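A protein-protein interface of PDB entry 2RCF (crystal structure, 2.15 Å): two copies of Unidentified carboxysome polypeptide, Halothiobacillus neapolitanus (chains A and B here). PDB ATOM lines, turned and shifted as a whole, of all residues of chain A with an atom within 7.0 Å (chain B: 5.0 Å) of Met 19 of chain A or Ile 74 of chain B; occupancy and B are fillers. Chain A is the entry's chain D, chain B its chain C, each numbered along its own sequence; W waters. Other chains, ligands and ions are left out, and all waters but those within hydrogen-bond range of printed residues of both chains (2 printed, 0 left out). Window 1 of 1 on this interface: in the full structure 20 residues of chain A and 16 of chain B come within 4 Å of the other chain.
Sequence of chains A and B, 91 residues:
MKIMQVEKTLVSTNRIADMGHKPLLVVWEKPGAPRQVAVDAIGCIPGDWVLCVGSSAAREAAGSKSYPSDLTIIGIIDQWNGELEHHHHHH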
ATOM      1  N   SER A  12       0.368  17.857 -13.710  1.00  0.00           N
ATOM      2  CA  SER A  12       0.288  18.931 -12.730  1.00  0.00           C
ATOM      3  C   SER A  12      -1.018  18.768 -11.969  1.00  0.00           C
ATOM      4  O   SER A  12      -2.066  19.235 -12.417  1.00  0.00           O
ATOM      5  CB  SER A  12       0.335  20.296 -13.421  1.00  0.00           C
ATOM      6  OG  SER A  12       0.275  21.353 -12.476  1.00  0.00           O
ATOM      7  N   ASN A  14      -1.648  19.905  -8.785  1.00  0.00           N
ATOM      8  CA  ASN A  14      -1.934  21.204  -8.181  1.00  0.00           C
ATOM      9  C   ASN A  14      -1.882  22.306  -9.239  1.00  0.00           C
ATOM     10  O   ASN A  14      -0.822  22.876  -9.508  1.00  0.00           O
ATOM     11  CB  ASN A  14      -0.947  21.491  -7.038  1.00  0.00           C
ATOM     12  CG  ASN A  14      -1.378  22.657  -6.156  1.00  0.00           C
ATOM     13  OD1 ASN A  14      -2.468  23.207  -6.310  1.00  0.00           O
ATOM     14  ND2 ASN A  14      -0.514  23.036  -5.222  1.00  0.00           N
ATOM     15  N   ARG A  15      -3.036  22.580  -9.845  1.00  0.00           N
ATOM     16  CA  ARG A  15      -3.179  23.647 -10.831  1.00  0.00           C
ATOM     17  C   ARG A  15      -4.492  24.404 -10.607  1.00  0.00           C
ATOM     18  O   ARG A  15      -5.380  23.920  -9.895  1.00  0.00           O
ATOM     19  CB  ARG A  15      -3.109  23.071 -12.245  1.00  0.00           C
ATOM     20  CG  ARG A  15      -4.337  22.279 -12.681  1.00  0.00           C
ATOM     21  CD  ARG A  15      -3.993  21.304 -13.805  1.00  0.00           C
ATOM     22  NE  ARG A  15      -5.048  21.197 -14.806  1.00  0.00           N
ATOM     23  CZ  ARG A  15      -5.006  20.394 -15.868  1.00  0.00           C
ATOM     24  NH1 ARG A  15      -3.963  19.594 -16.077  1.00  0.00           N
ATOM     25  NH2 ARG A  15      -6.020  20.390 -16.726  1.00  0.00           N
ATOM     26  N   ILE A  16      -4.610  25.593 -11.203  1.00  0.00           N
ATOM     27  CA  ILE A  16      -5.795  26.435 -10.995  1.00  0.00           C
ATOM     28  C   ILE A  16      -7.053  25.771 -11.557  1.00  0.00           C
ATOM     29  O   ILE A  16      -6.979  24.972 -12.495  1.00  0.00           O
ATOM     30  CB  ILE A  16      -5.631  27.871 -11.579  1.00  0.00           C
ATOM     31  CG1 ILE A  16      -5.562  27.858 -13.112  1.00  0.00           C
ATOM     32  CG2 ILE A  16      -4.398  28.545 -10.992  1.00  0.00           C
ATOM     33  CD1 ILE A  16      -5.494  29.243 -13.722  1.00  0.00           C
ATOM     34  N   ALA A  17      -8.201  26.106 -10.970  1.00  0.00           N
ATOM     35  CA  ALA A  17      -9.476  25.471 -11.317  1.00  0.00           C
ATOM     36  C   ALA A  17      -9.893  25.747 -12.763  1.00  0.00           C
ATOM     37  O   ALA A  17     -10.490  24.886 -13.415  1.00  0.00           O
ATOM     38  CB  ALA A  17     -10.572  25.920 -10.351  1.00  0.00           C
ATOM     39  N   ASP A  18      -9.553  26.936 -13.258  1.00  0.00           N
ATOM     40  CA  ASP A  18      -9.871  27.360 -14.627  1.00  0.00           C
ATOM     41  C   ASP A  18      -9.356  26.425 -15.725  1.00  0.00           C
ATOM     42  O   ASP A  18      -9.854  26.459 -16.847  1.00  0.00           O
ATOM     43  CB  ASP A  18      -9.318  28.772 -14.886  1.00  0.00           C
ATOM     44  CG  ASP A  18     -10.121  29.862 -14.191  1.00  0.00           C
ATOM     45  OD1 ASP A  18      -9.541  30.937 -13.919  1.00  0.00           O
ATOM     46  OD2 ASP A  18     -11.326  29.656 -13.923  1.00  0.00           O
ATOM     47  N   MET A  19      -8.359  25.603 -15.405  1.00  0.00           N
ATOM     48  CA  MET A  19      -7.786  24.662 -16.368  1.00  0.00           C
ATOM     49  C   MET A  19      -8.705  23.478 -16.708  1.00  0.00           C
ATOM     50  O   MET A  19      -8.487  22.796 -17.707  1.00  0.00           O
ATOM     51  CB  MET A  19      -6.442  24.147 -15.849  1.00  0.00           C
ATOM     52  CG  MET A  19      -5.414  25.259 -15.603  1.00  0.00           C
ATOM     53  SD  MET A  19      -3.711  24.741 -15.887  1.00  0.00           S
ATOM     54  CE  MET A  19      -3.740  24.495 -17.661  1.00  0.00           C
ATOM     55  N   GLY A  20      -9.726  23.235 -15.891  1.00  0.00           N
ATOM     56  CA  GLY A  20     -10.635  22.110 -16.116  1.00  0.00           C
ATOM     57  C   GLY A  20      -9.895  20.782 -16.150  1.00  0.00           C
ATOM     58  O   GLY A  20      -8.962  20.569 -15.375  1.00  0.00           O
ATOM     59  N   HIS A  21     -10.301  19.897 -17.057  1.00  0.00           N
ATOM     60  CA  HIS A  21      -9.680  18.572 -17.189  1.00  0.00           C
ATOM     61  C   HIS A  21      -8.963  18.385 -18.531  1.00  0.00           C
ATOM     62  O   HIS A  21      -8.693  17.254 -18.942  1.00  0.00           O
ATOM     63  CB  HIS A  21     -10.729  17.473 -17.008  1.00  0.00           C
ATOM     64  CG  HIS A  21     -11.832  17.512 -18.020  1.00  0.00           C
ATOM     65  ND1 HIS A  21     -11.642  17.183 -19.346  1.00  0.00           N
ATOM     66  CD2 HIS A  21     -13.144  17.829 -17.894  1.00  0.00           C
ATOM     67  CE1 HIS A  21     -12.788  17.301 -19.993  1.00  0.00           C
ATOM     68  NE2 HIS A  21     -13.715  17.688 -19.135  1.00  0.00           N
ATOM     69  N   LYS A  22      -8.647  19.491 -19.201  1.00  0.00           N
ATOM     70  CA  LYS A  22      -8.034  19.430 -20.522  1.00  0.00           C
ATOM     71  C   LYS A  22      -6.612  18.892 -20.391  1.00  0.00           C
ATOM     72  O   LYS A  22      -5.881  19.311 -19.502  1.00  0.00           O
ATOM     73  CB  LYS A  22      -8.019  20.817 -21.170  1.00  0.00           C
ATOM     74  CG  LYS A  22      -9.383  21.493 -21.172  1.00  0.00           C
ATOM     75  CD  LYS A  22      -9.472  22.628 -22.180  1.00  0.00           C
ATOM     76  CE  LYS A  22     -10.829  23.318 -22.078  1.00  0.00           C
ATOM     77  NZ  LYS A  22     -11.869  22.561 -22.821  1.00  0.00           N
ATOM     78  N   PRO A  23      -6.213  17.953 -21.267  1.00  0.00           N
ATOM     79  CA  PRO A  23      -4.858  17.407 -21.155  1.00  0.00           C
ATOM     80  C   PRO A  23      -3.774  18.426 -21.526  1.00  0.00           C
ATOM     81  O   PRO A  23      -3.960  19.230 -22.443  1.00  0.00           O
ATOM     82  CB  PRO A  23      -4.850  16.224 -22.128  1.00  0.00           C
ATOM     83  CG  PRO A  23      -6.094  16.310 -22.925  1.00  0.00           C
ATOM     84  CD  PRO A  23      -6.975  17.377 -22.389  1.00  0.00           C
ATOM     85  N   LEU A  24      -2.665  18.391 -20.789  1.00  0.00           N
ATOM     86  CA  LEU A  24      -1.511  19.227 -21.070  1.00  0.00           C
ATOM     87  C   LEU A  24      -0.391  18.312 -21.532  1.00  0.00           C
ATOM     88  O   LEU A  24      -0.132  17.270 -20.907  1.00  0.00           O
ATOM     89  CB  LEU A  24      -1.075  19.998 -19.824  1.00  0.00           C
ATOM     90  CG  LEU A  24      -2.140  20.867 -19.154  1.00  0.00           C
ATOM     91  CD1 LEU A  24      -1.631  21.362 -17.824  1.00  0.00           C
ATOM     92  CD2 LEU A  24      -2.541  22.036 -20.058  1.00  0.00           C
ATOM     93  N   VAL A  37       4.712  23.709 -23.025  1.00  0.00           N
ATOM     94  CA  VAL A  37       3.509  22.952 -22.690  1.00  0.00           C
ATOM     95  C   VAL A  37       2.295  23.511 -23.422  1.00  0.00           C
ATOM     96  O   VAL A  37       2.067  24.720 -23.429  1.00  0.00           O
ATOM     97  CB  VAL A  37       3.225  22.964 -21.165  1.00  0.00           C
ATOM     98  CG1 VAL A  37       1.926  22.221 -20.858  1.00  0.00           C
ATOM     99  CG2 VAL A  37       4.401  22.361 -20.384  1.00  0.00           C
ATOM    100  N   VAL A  39      -2.080  22.896 -24.282  1.00  0.00           N
ATOM    101  CA  VAL A  39      -3.322  22.154 -24.060  1.00  0.00           C
ATOM    102  C   VAL A  39      -3.685  21.409 -25.341  1.00  0.00           C
ATOM    103  O   VAL A  39      -3.586  21.945 -26.453  1.00  0.00           O
ATOM    104  CB  VAL A  39      -4.523  22.989 -23.477  1.00  0.00           C
ATOM    105  CG1 VAL A  39      -4.213  24.457 -23.372  1.00  0.00           C
ATOM    106  CG2 VAL A  39      -5.833  22.731 -24.250  1.00  0.00           C
ATOM    107  N   TYR A  67     -10.304  30.624 -21.243  1.00  0.00           N
ATOM    108  CA  TYR A  67      -9.432  29.507 -20.866  1.00  0.00           C
ATOM    109  C   TYR A  67      -7.965  29.955 -20.743  1.00  0.00           C
ATOM    110  O   TYR A  67      -7.464  30.660 -21.614  1.00  0.00           O
ATOM    111  CB  TYR A  67      -9.544  28.329 -21.840  1.00  0.00           C
ATOM    112  CG  TYR A  67      -8.865  27.107 -21.275  1.00  0.00           C
ATOM    113  CD1 TYR A  67      -7.508  26.893 -21.475  1.00  0.00           C
ATOM    114  CD2 TYR A  67      -9.565  26.200 -20.483  1.00  0.00           C
ATOM    115  CE1 TYR A  67      -6.868  25.802 -20.931  1.00  0.00           C
ATOM    116  CE2 TYR A  67      -8.931  25.093 -19.930  1.00  0.00           C
ATOM    117  CZ  TYR A  67      -7.576  24.905 -20.159  1.00  0.00           C
ATOM    118  OH  TYR A  67      -6.923  23.818 -19.635  1.00  0.00           O
ATOM    119  N   PRO A  68      -7.273  29.544 -19.660  1.00  0.00           N
ATOM    120  CA  PRO A  68      -5.869  29.929 -19.470  1.00  0.00           C
ATOM    121  C   PRO A  68      -4.883  29.117 -20.321  1.00  0.00           C
ATOM    122  O   PRO A  68      -4.243  28.182 -19.828  1.00  0.00           O
ATOM    123  CB  PRO A  68      -5.645  29.683 -17.973  1.00  0.00           C
ATOM    124  CG  PRO A  68      -6.542  28.545 -17.662  1.00  0.00           C
ATOM    125  CD  PRO A  68      -7.758  28.715 -18.538  1.00  0.00           C
ATOM    126  N   SER A  69      -4.766  29.488 -21.591  1.00  0.00           N
ATOM    127  CA  SER A  69      -3.790  28.883 -22.489  1.00  0.00           C
ATOM    128  C   SER A  69      -3.171  29.945 -23.381  1.00  0.00           C
ATOM    129  O   SER A  69      -3.864  30.843 -23.868  1.00  0.00           O
ATOM    130  CB  SER A  69      -4.441  27.798 -23.359  1.00  0.00           C
ATOM    131  OG  SER A  69      -3.462  27.090 -24.116  1.00  0.00           O
ATOM    132  N   MET B   1       2.708  27.549 -23.106  1.00  0.00           N
ATOM    133  CA  MET B   1       3.087  27.703 -21.670  1.00  0.00           C
ATOM    134  C   MET B   1       4.519  27.222 -21.452  1.00  0.00           C
ATOM    135  O   MET B   1       5.027  26.390 -22.210  1.00  0.00           O
ATOM    136  CB  MET B   1       2.127  26.921 -20.770  1.00  0.00           C
ATOM    137  CG  MET B   1       0.735  27.529 -20.652  1.00  0.00           C
ATOM    138  SD  MET B   1      -0.474  26.858 -21.804  1.00  0.00           S
ATOM    139  CE  MET B   1       0.321  27.073 -23.355  1.00  0.00           C
ATOM    140  N   ILE B  42      -0.969  30.028  -7.501  1.00  0.00           N
ATOM    141  CA  ILE B  42      -1.074  28.694  -6.903  1.00  0.00           C
ATOM    142  C   ILE B  42      -0.621  28.681  -5.444  1.00  0.00           C
ATOM    143  O   ILE B  42      -1.280  28.088  -4.585  1.00  0.00           O
ATOM    144  CB  ILE B  42      -0.239  27.662  -7.702  1.00  0.00           C
ATOM    145  CG1 ILE B  42      -0.949  27.301  -9.004  1.00  0.00           C
ATOM    146  CG2 ILE B  42      -0.020  26.386  -6.891  1.00  0.00           C
ATOM    147  CD1 ILE B  42      -2.196  26.441  -8.799  1.00  0.00           C
ATOM    148  N   LEU B  51       4.263  25.706 -13.972  1.00  0.00           N
ATOM    149  CA  LEU B  51       3.720  25.929 -15.304  1.00  0.00           C
ATOM    150  C   LEU B  51       3.270  27.383 -15.379  1.00  0.00           C
ATOM    151  O   LEU B  51       2.464  27.820 -14.564  1.00  0.00           O
ATOM    152  CB  LEU B  51       2.542  24.987 -15.549  1.00  0.00           C
ATOM    153  CG  LEU B  51       1.940  24.963 -16.951  1.00  0.00           C
ATOM    154  CD1 LEU B  51       2.953  24.457 -17.974  1.00  0.00           C
ATOM    155  CD2 LEU B  51       0.694  24.088 -16.954  1.00  0.00           C
ATOM    156  N   CYS B  52       3.805  28.121 -16.349  1.00  0.00           N
ATOM    157  CA  CYS B  52       3.534  29.545 -16.505  1.00  0.00           C
ATOM    158  C   CYS B  52       2.835  29.816 -17.830  1.00  0.00           C
ATOM    159  O   CYS B  52       3.219  29.258 -18.860  1.00  0.00           O
ATOM    160  CB  CYS B  52       4.841  30.334 -16.468  1.00  0.00           C
ATOM    161  SG  CYS B  52       5.754  30.189 -14.919  1.00  0.00           S
ATOM    162  N   VAL B  53       1.817  30.674 -17.791  1.00  0.00           N
ATOM    163  CA  VAL B  53       1.106  31.098 -18.994  1.00  0.00           C
ATOM    164  C   VAL B  53       1.315  32.598 -19.202  1.00  0.00           C
ATOM    165  O   VAL B  53       1.356  33.368 -18.239  1.00  0.00           O
ATOM    166  CB  VAL B  53      -0.411  30.761 -18.921  1.00  0.00           C
ATOM    167  CG1 VAL B  53      -1.133  31.631 -17.878  1.00  0.00           C
ATOM    168  CG2 VAL B  53      -1.055  30.907 -20.290  1.00  0.00           C
ATOM    169  N   ALA B  61      -5.977  34.396 -15.561  1.00  0.00           N
ATOM    170  CA  ALA B  61      -5.279  33.393 -14.758  1.00  0.00           C
ATOM    171  C   ALA B  61      -4.855  33.956 -13.403  1.00  0.00           C
ATOM    172  O   ALA B  61      -4.878  33.246 -12.410  1.00  0.00           O
ATOM    173  CB  ALA B  61      -4.067  32.854 -15.503  1.00  0.00           C
ATOM    174  N   THR B  72       1.844  34.330 -15.628  1.00  0.00           N
ATOM    175  CA  THR B  72       1.186  33.880 -14.410  1.00  0.00           C
ATOM    176  C   THR B  72       1.433  32.396 -14.167  1.00  0.00           C
ATOM    177  O   THR B  72       1.325  31.589 -15.086  1.00  0.00           O
ATOM    178  CB  THR B  72      -0.325  34.165 -14.460  1.00  0.00           C
ATOM    179  OG1 THR B  72      -0.537  35.578 -14.612  1.00  0.00           O
ATOM    180  CG2 THR B  72      -1.009  33.687 -13.173  1.00  0.00           C
ATOM    181  N   ILE B  73       1.768  32.055 -12.924  1.00  0.00           N
ATOM    182  CA  ILE B  73       1.926  30.661 -12.509  1.00  0.00           C
ATOM    183  C   ILE B  73       0.548  30.047 -12.282  1.00  0.00           C
ATOM    184  O   ILE B  73      -0.213  30.504 -11.422  1.00  0.00           O
ATOM    185  CB  ILE B  73       2.744  30.533 -11.207  1.00  0.00           C
ATOM    186  CG1 ILE B  73       4.153  31.110 -11.392  1.00  0.00           C
ATOM    187  CG2 ILE B  73       2.837  29.076 -10.767  1.00  0.00           C
ATOM    188  CD1 ILE B  73       4.952  31.189 -10.091  1.00  0.00           C
ATOM    189  N   ILE B  74       0.234  29.013 -13.058  1.00  0.00           N
ATOM    190  CA  ILE B  74      -1.093  28.402 -13.037  1.00  0.00           C
ATOM    191  C   ILE B  74      -1.070  26.937 -12.594  1.00  0.00           C
ATOM    192  O   ILE B  74      -2.120  26.295 -12.527  1.00  0.00           O
ATOM    193  CB  ILE B  74      -1.781  28.515 -14.421  1.00  0.00           C
ATOM    194  CG1 ILE B  74      -1.008  27.743 -15.496  1.00  0.00           C
ATOM    195  CG2 ILE B  74      -1.908  29.983 -14.815  1.00  0.00           C
ATOM    196  CD1 ILE B  74      -1.672  27.771 -16.865  1.00  0.00           C
ATOM    197  N   GLY B  75       0.120  26.417 -12.293  1.00  0.00           N
ATOM    198  CA  GLY B  75       0.262  25.047 -11.834  1.00  0.00           C
ATOM    199  C   GLY B  75       1.641  24.740 -11.280  1.00  0.00           C
ATOM    200  O   GLY B  75       2.624  25.386 -11.643  1.00  0.00           O
ATOM    201  N   ILE B  76       1.700  23.759 -10.383  1.00  0.00           N
ATOM    202  CA  ILE B  76       2.969  23.210  -9.912  1.00  0.00           C
ATOM    203  C   ILE B  76       3.168  21.855 -10.568  1.00  0.00           C
ATOM    204  O   ILE B  76       2.261  21.026 -10.571  1.00  0.00           O
ATOM    205  CB  ILE B  76       3.005  23.091  -8.381  1.00  0.00           C
ATOM    206  CG1 ILE B  76       3.087  24.487  -7.767  1.00  0.00           C
ATOM    207  CG2 ILE B  76       4.203  22.257  -7.928  1.00  0.00           C
ATOM    208  CD1 ILE B  76       2.932  24.504  -6.280  1.00  0.00           C
HETATM  209  O   HOH W   1       0.938  19.424  -8.681  1.00  0.00           O
HETATM  210  O   HOH W   2      -8.253  31.922 -16.183  1.00  0.00           O
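Water W1 lies within hydrogen-bond range of the backbone NH of Asn 14 of chain A (2.6 Å) and the backbone carbonyl oxygen of Ile 76 of chain B (2.8 Å). Water W2 lies within hydrogen-bond range of the side-chain carboxylate of Asp 18 of chain A (2.8 Å) and the backbone NH of Ala 61 of chain B (3.4 Å).
Asn 14 of chain A touches Ile 42 of chain B (ND2 to CG2, 3.8 Å). Asn 14 of chain A touches Gly 75 of chain B. Arg 15 of chain A touches Ile 42 of chain B. Ile 74 of chain B touches Arg 15 of chain A. N of Ile 16 of chain A touches CD1 of Ile 42 of chain B, 3.5 Å away. SD of Met 19 of chain A touches CD1 of Ile 74 of chain B, at 3.8 Å. Leu 51 of chain B touches Leu 24 of chain A. Leu 51 of chain B touches Val 37 of chain A. Ile 74 of chain B touches Pro 68 of chain A (CD1 to O, 3.9 Å). Ser 69 of chain A touches Val 53 of chain B (C to CG2, 3.9 Å).
Of chain B, only Ile 74 (3.8 Å) comes within 4 Å of Met 19 of chain A. Ile 74 of chain B touches four residues of chain A. Of the printed residues of chain B, Leu 24 of chain A touches Leu 51. Of the printed residues of chain B, Asn 14 of chain A touches Ile 42, Gly 75 and Ile 76. Printed residues of chain A within 4 Å of Leu 51 of chain B: Leu 24 (3.7 Å) and Val 37 (3.5 Å). The nearest residue of chain A that does not touch Ile 74 of chain B is Asn 14 of chain A (4.7 Å). The nearest printed residue of chain B that does not touch Asn 14 of chain A is Ile 74 of chain B (4.7 Å).
No position is printed for both chains.
Of the 11 printed residues of chain B, 7 touch a printed residue of chain A. Printed residues of chain B that touch a printed residue of chain A: Met 1, Ile 42, Leu 51, Val 53, Ile 74, Gly 75 and Ile 76. Hydrophobic or aromatic side chains of chain A within 4 Å of the printed part of chain B: Ile 16, Met 19, Leu 24 and Val 37. Among the printed residues, 17 pairs touch across the chains. Among the printed residues, no Asp or Glu carboxylate lies within 4 Å of a Lys or Arg side-chain nitrogen of the other chain.
The guanidinium group of Arg 15 of chain A lies within hydrogen-bond range of the backbone carbonyl oxygen of Lys 22 of chain A. The backbone carbonyl oxygen of Gly 20 of chain A is in hydrogen-bond range of the guanidinium group of Arg 15 of chain A (3.2 Å). O of Val 53 of chain B sits at hydrogen-bond distance from N of Thr 72 of chain B, 2.8 Å away. The backbone NH (N) of Leu 51 of chain B is in hydrogen-bond range of the backbone carbonyl oxygen (O) of Gly 75 of chain B (2.9 Å). OH of Tyr 67 of chain A lies within hydrogen-bond range of O of Met 19 of chain A, at 2.7 Å. The backbone NH of Ile 74 of chain B sits at hydrogen-bond distance from the backbone carbonyl oxygen of Leu 51 of chain B (2.9 Å).
N of Ile 76 of chain B sits at hydrogen-bond distance from O of Asn 14 of chain A (2.8 Å). The side-chain sulfur of Met 1 of chain B lies within hydrogen-bond range of the side-chain hydroxyl of Ser 69 of chain A (3.8 Å). O of Ile 74 of chain B is in hydrogen-bond range of N of Ile 16 of chain A. O of Ile 76 of chain B lies within hydrogen-bond range of OG of Ser 12 of chain A (2.8 Å). The backbone carbonyl oxygen (O) of Met 1 of chain B lies within hydrogen-bond range of the backbone NH (N) of Val 37 of chain A (2.8 Å).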
